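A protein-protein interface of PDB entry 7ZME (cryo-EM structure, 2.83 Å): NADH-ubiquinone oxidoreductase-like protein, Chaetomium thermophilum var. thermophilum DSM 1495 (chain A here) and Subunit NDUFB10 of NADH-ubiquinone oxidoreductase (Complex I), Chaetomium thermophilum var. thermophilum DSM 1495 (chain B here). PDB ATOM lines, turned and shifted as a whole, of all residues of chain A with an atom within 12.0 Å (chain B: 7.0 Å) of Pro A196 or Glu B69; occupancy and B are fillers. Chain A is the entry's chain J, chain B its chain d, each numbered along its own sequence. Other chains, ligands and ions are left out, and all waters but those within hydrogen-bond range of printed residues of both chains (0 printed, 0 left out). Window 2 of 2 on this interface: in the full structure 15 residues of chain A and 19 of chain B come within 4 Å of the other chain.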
ATOM      1  N   PRO A 191      17.735  32.093 -15.601  1.00  0.00           N
ATOM      2  CA  PRO A 191      16.446  31.498 -15.976  1.00  0.00           C
ATOM      3  C   PRO A 191      16.018  30.402 -15.008  1.00  0.00           C
ATOM      4  O   PRO A 191      16.846  29.708 -14.413  1.00  0.00           O
ATOM      5  CB  PRO A 191      16.708  30.922 -17.373  1.00  0.00           C
ATOM      6  CG  PRO A 191      18.033  31.469 -17.819  1.00  0.00           C
ATOM      7  CD  PRO A 191      18.561  32.398 -16.779  1.00  0.00           C
ATOM      8  N   VAL A 192      14.701  30.253 -14.858  1.00  0.00           N
ATOM      9  CA  VAL A 192      14.119  29.321 -13.895  1.00  0.00           C
ATOM     10  C   VAL A 192      14.450  27.878 -14.251  1.00  0.00           C
ATOM     11  O   VAL A 192      14.889  27.582 -15.368  1.00  0.00           O
ATOM     12  CB  VAL A 192      12.596  29.516 -13.788  1.00  0.00           C
ATOM     13  CG1 VAL A 192      12.278  30.877 -13.198  1.00  0.00           C
ATOM     14  CG2 VAL A 192      11.941  29.353 -15.154  1.00  0.00           C
ATOM     15  N   CYS A 193      14.230  26.973 -13.299  1.00  0.00           N
ATOM     16  CA  CYS A 193      14.610  25.573 -13.428  1.00  0.00           C
ATOM     17  C   CYS A 193      13.517  24.713 -14.057  1.00  0.00           C
ATOM     18  O   CYS A 193      13.671  23.490 -14.106  1.00  0.00           O
ATOM     19  CB  CYS A 193      14.995  25.013 -12.051  1.00  0.00           C
ATOM     20  SG  CYS A 193      15.888  23.435 -12.060  1.00  0.00           S
ATOM     21  N   ALA A 194      12.389  25.310 -14.449  1.00  0.00           N
ATOM     22  CA  ALA A 194      11.426  24.731 -15.388  1.00  0.00           C
ATOM     23  C   ALA A 194      11.112  23.257 -15.160  1.00  0.00           C
ATOM     24  O   ALA A 194      10.732  22.552 -16.102  1.00  0.00           O
ATOM     25  CB  ALA A 194      11.918  24.927 -16.825  1.00  0.00           C
ATOM     26  N   ASP A 195      11.246  22.784 -13.924  1.00  0.00           N
ATOM     27  CA  ASP A 195      11.037  21.374 -13.618  1.00  0.00           C
ATOM     28  C   ASP A 195      10.936  21.182 -12.110  1.00  0.00           C
ATOM     29  O   ASP A 195      11.805  21.655 -11.367  1.00  0.00           O
ATOM     30  CB  ASP A 195      12.176  20.528 -14.194  1.00  0.00           C
ATOM     31  CG  ASP A 195      12.089  19.072 -13.784  1.00  0.00           C
ATOM     32  OD1 ASP A 195      10.969  18.525 -13.742  1.00  0.00           O
ATOM     33  OD2 ASP A 195      13.147  18.470 -13.502  1.00  0.00           O
ATOM     34  N   PRO A 196       9.894  20.505 -11.619  1.00  0.00           N
ATOM     35  CA  PRO A 196       9.816  20.243 -10.172  1.00  0.00           C
ATOM     36  C   PRO A 196      11.004  19.463  -9.636  1.00  0.00           C
ATOM     37  O   PRO A 196      11.451  19.717  -8.512  1.00  0.00           O
ATOM     38  CB  PRO A 196       8.506  19.456 -10.035  1.00  0.00           C
ATOM     39  CG  PRO A 196       7.696  19.883 -11.208  1.00  0.00           C
ATOM     40  CD  PRO A 196       8.674  20.079 -12.325  1.00  0.00           C
ATOM     41  N   ASP A 197      11.529  18.517 -10.411  1.00  0.00           N
ATOM     42  CA  ASP A 197      12.701  17.773  -9.982  1.00  0.00           C
ATOM     43  C   ASP A 197      13.965  18.609 -10.173  1.00  0.00           C
ATOM     44  O   ASP A 197      13.964  19.639 -10.853  1.00  0.00           O
ATOM     45  CB  ASP A 197      12.818  16.458 -10.754  1.00  0.00           C
ATOM     46  N   GLN A 198      15.050  18.146  -9.557  1.00  0.00           N
ATOM     47  CA  GLN A 198      16.352  18.807  -9.633  1.00  0.00           C
ATOM     48  C   GLN A 198      16.279  20.262  -9.178  1.00  0.00           C
ATOM     49  O   GLN A 198      16.221  20.545  -7.981  1.00  0.00           O
ATOM     50  CB  GLN A 198      16.914  18.731 -11.056  1.00  0.00           C
ATOM     51  N   GLU B  63      -2.147  14.082 -18.079  1.00  0.00           N
ATOM     52  CA  GLU B  63      -2.091  14.430 -16.665  1.00  0.00           C
ATOM     53  C   GLU B  63      -3.173  15.431 -16.272  1.00  0.00           C
ATOM     54  O   GLU B  63      -3.856  15.241 -15.262  1.00  0.00           O
ATOM     55  CB  GLU B  63      -0.706  14.977 -16.315  1.00  0.00           C
ATOM     56  CG  GLU B  63       0.363  13.903 -16.175  1.00  0.00           C
ATOM     57  CD  GLU B  63      -0.134  12.647 -15.482  1.00  0.00           C
ATOM     58  OE1 GLU B  63      -0.689  12.744 -14.369  1.00  0.00           O
ATOM     59  OE2 GLU B  63       0.028  11.552 -16.060  1.00  0.00           O
ATOM     60  N   VAL B  65      -4.677  18.278 -14.507  1.00  0.00           N
ATOM     61  CA  VAL B  65      -4.377  19.120 -13.353  1.00  0.00           C
ATOM     62  C   VAL B  65      -2.911  19.000 -12.970  1.00  0.00           C
ATOM     63  O   VAL B  65      -2.202  20.002 -12.820  1.00  0.00           O
ATOM     64  CB  VAL B  65      -5.290  18.744 -12.174  1.00  0.00           C
ATOM     65  CG1 VAL B  65      -4.915  19.516 -10.955  1.00  0.00           C
ATOM     66  CG2 VAL B  65      -6.697  19.066 -12.510  1.00  0.00           C
ATOM     67  N   ASN B  66      -2.436  17.771 -12.813  1.00  0.00           N
ATOM     68  CA  ASN B  66      -1.065  17.510 -12.387  1.00  0.00           C
ATOM     69  C   ASN B  66      -0.109  17.333 -13.564  1.00  0.00           C
ATOM     70  O   ASN B  66       0.658  16.379 -13.631  1.00  0.00           O
ATOM     71  CB  ASN B  66      -1.051  16.306 -11.452  1.00  0.00           C
ATOM     72  CG  ASN B  66      -1.517  15.027 -12.125  1.00  0.00           C
ATOM     73  OD1 ASN B  66      -1.750  14.990 -13.330  1.00  0.00           O
ATOM     74  ND2 ASN B  66      -1.657  13.967 -11.338  1.00  0.00           N
ATOM     75  N   HIS B  67      -0.133  18.283 -14.498  1.00  0.00           N
ATOM     76  CA  HIS B  67       0.874  18.340 -15.546  1.00  0.00           C
ATOM     77  C   HIS B  67       2.058  19.198 -15.144  1.00  0.00           C
ATOM     78  O   HIS B  67       3.174  18.966 -15.617  1.00  0.00           O
ATOM     79  CB  HIS B  67       0.284  18.902 -16.844  1.00  0.00           C
ATOM     80  CG  HIS B  67       0.118  20.390 -16.842  1.00  0.00           C
ATOM     81  ND1 HIS B  67       1.090  21.241 -17.322  1.00  0.00           N
ATOM     82  CD2 HIS B  67      -0.890  21.180 -16.407  1.00  0.00           C
ATOM     83  CE1 HIS B  67       0.682  22.489 -17.195  1.00  0.00           C
ATOM     84  NE2 HIS B  67      -0.515  22.480 -16.638  1.00  0.00           N
ATOM     85  N   LEU B  68       1.827  20.179 -14.271  1.00  0.00           N
ATOM     86  CA  LEU B  68       2.877  21.069 -13.808  1.00  0.00           C
ATOM     87  C   LEU B  68       3.858  20.378 -12.876  1.00  0.00           C
ATOM     88  O   LEU B  68       4.911  20.950 -12.581  1.00  0.00           O
ATOM     89  CB  LEU B  68       2.253  22.280 -13.119  1.00  0.00           C
ATOM     90  CG  LEU B  68       1.874  23.422 -14.058  1.00  0.00           C
ATOM     91  CD1 LEU B  68       1.351  24.614 -13.283  1.00  0.00           C
ATOM     92  CD2 LEU B  68       3.071  23.813 -14.910  1.00  0.00           C
ATOM     93  N   GLU B  69       3.550  19.167 -12.414  1.00  0.00           N
ATOM     94  CA  GLU B  69       4.466  18.418 -11.573  1.00  0.00           C
ATOM     95  C   GLU B  69       4.776  17.026 -12.093  1.00  0.00           C
ATOM     96  O   GLU B  69       5.520  16.292 -11.433  1.00  0.00           O
ATOM     97  CB  GLU B  69       3.918  18.311 -10.143  1.00  0.00           C
ATOM     98  CG  GLU B  69       2.817  17.291  -9.959  1.00  0.00           C
ATOM     99  CD  GLU B  69       2.613  16.929  -8.504  1.00  0.00           C
ATOM    100  OE1 GLU B  69       3.562  17.096  -7.709  1.00  0.00           O
ATOM    101  OE2 GLU B  69       1.501  16.486  -8.149  1.00  0.00           O
ATOM    102  N   LYS B  70       4.240  16.638 -13.248  1.00  0.00           N
ATOM    103  CA  LYS B  70       4.495  15.315 -13.788  1.00  0.00           C
ATOM    104  C   LYS B  70       5.029  15.331 -15.211  1.00  0.00           C
ATOM    105  O   LYS B  70       5.334  14.261 -15.749  1.00  0.00           O
ATOM    106  CB  LYS B  70       3.216  14.465 -13.737  1.00  0.00           C
ATOM    107  CG  LYS B  70       2.834  14.034 -12.332  1.00  0.00           C
ATOM    108  CD  LYS B  70       1.718  13.006 -12.351  1.00  0.00           C
ATOM    109  CE  LYS B  70       2.232  11.639 -12.767  1.00  0.00           C
ATOM    110  NZ  LYS B  70       1.130  10.644 -12.873  1.00  0.00           N
ATOM    111  N   CYS B  71       5.156  16.501 -15.834  1.00  0.00           N
ATOM    112  CA  CYS B  71       5.612  16.606 -17.214  1.00  0.00           C
ATOM    113  C   CYS B  71       6.766  17.591 -17.330  1.00  0.00           C
ATOM    114  O   CYS B  71       6.992  18.170 -18.396  1.00  0.00           O
ATOM    115  CB  CYS B  71       4.463  17.011 -18.139  1.00  0.00           C
ATOM    116  SG  CYS B  71       2.981  15.975 -18.035  1.00  0.00           S
ATOM    117  N   GLY B  72       7.507  17.792 -16.238  1.00  0.00           N
ATOM    118  CA  GLY B  72       8.611  18.734 -16.247  1.00  0.00           C
ATOM    119  C   GLY B  72       9.886  18.203 -16.854  1.00  0.00           C
ATOM    120  O   GLY B  72      10.742  18.996 -17.255  1.00  0.00           O
ATOM    121  N   LYS B  73      10.039  16.880 -16.924  1.00  0.00           N
ATOM    122  CA  LYS B  73      11.234  16.312 -17.537  1.00  0.00           C
ATOM    123  C   LYS B  73      11.333  16.705 -19.003  1.00  0.00           C
ATOM    124  O   LYS B  73      12.417  17.040 -19.493  1.00  0.00           O
ATOM    125  CB  LYS B  73      11.227  14.790 -17.386  1.00  0.00           C
ATOM    126  CG  LYS B  73      12.473  14.110 -17.926  1.00  0.00           C
ATOM    127  CD  LYS B  73      13.704  14.516 -17.135  1.00  0.00           C
ATOM    128  CE  LYS B  73      13.607  14.048 -15.693  1.00  0.00           C
ATOM    129  NZ  LYS B  73      13.688  12.566 -15.585  1.00  0.00           N
ATOM    130  N   ARG B  75       9.756  19.347 -20.226  1.00  0.00           N
ATOM    131  CA  ARG B  75       9.733  20.803 -20.309  1.00  0.00           C
ATOM    132  C   ARG B  75      11.137  21.386 -20.372  1.00  0.00           C
ATOM    133  O   ARG B  75      11.389  22.312 -21.149  1.00  0.00           O
ATOM    134  CB  ARG B  75       8.948  21.385 -19.137  1.00  0.00           C
ATOM    135  CG  ARG B  75       7.453  21.368 -19.363  1.00  0.00           C
ATOM    136  CD  ARG B  75       6.725  22.189 -18.327  1.00  0.00           C
ATOM    137  NE  ARG B  75       6.043  21.340 -17.361  1.00  0.00           N
ATOM    138  CZ  ARG B  75       6.406  21.220 -16.091  1.00  0.00           C
ATOM    139  NH1 ARG B  75       5.733  20.417 -15.285  1.00  0.00           N
ATOM    140  NH2 ARG B  75       7.454  21.881 -15.633  1.00  0.00           N
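NH2 of Arg B75 is in hydrogen-bond range of O of Ala A194 (3.4 Å).
The backbone NH (N) of Asp A197 lies close to the side-chain carboxylate (OD1) of Asp A195 (3.4 Å). The guanidinium group (NH1) of Arg B75 sits at hydrogen-bond distance from the backbone carbonyl oxygen (O) of His B67 (3.0 Å). The guanidinium group of Arg B75 lies within hydrogen-bond range of the backbone carbonyl oxygen of Leu B68, 2.9 Å away. O of Cys B71 sits close to NE of Arg B75, 3.5 Å away.
Ala A194 touches Gly B72. Gly B72 touches Asp A195 (C to OD1, 3.3 Å). Asp A195 touches Lys B73 (OD1 to N, 3.7 Å). CG of Pro A196 touches O of Leu B68, at 3.3 Å. CA of Glu B69 touches CG of Pro A196 (3.6 Å). CD of Pro A196 touches NH2 of Arg B75, at 3.96 Å.
Of chain B, only Leu B68 (3.3 Å), Glu B69 (3.6 Å) and Arg B75 (3.96 Å) come within 4 Å of Pro A196. Glu B69 touches one residue of chain A. Of chain A, only Pro A196 comes within 4 Å of Leu B68. No residue of chain A comes within 4 Å of Lys B70. No residue of chain A comes within 4 Å of Cys B71. Of the printed residues of chain A, Gly B72 touches Ala A194 (3.7 Å) and Asp A195 (3.3 Å). Of the printed residues of chain A, Arg B75 touches Ala A194 and Pro A196. Printed residues of chain B within 4 Å of Ala A194: Gly B72 (3.7 Å) and Arg B75 (3.4 Å). Cys A193 touches none of the printed residues of chain B. Glu B63 touches none of the printed residues of chain A. The nearest residue of chain A that does not touch Glu B69 is Asp A195 (6.3 Å). The nearest printed residue of chain A that does not touch Lys B73 is Asp A197 (5.6 Å).
Printed residues of chain A that touch a printed residue of chain B: Ala A194, Asp A195 and Pro A196. Among the printed residues, no Asp or Glu carboxylate lies within 4 Å of a Lys or Arg side-chain nitrogen of the other chain.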
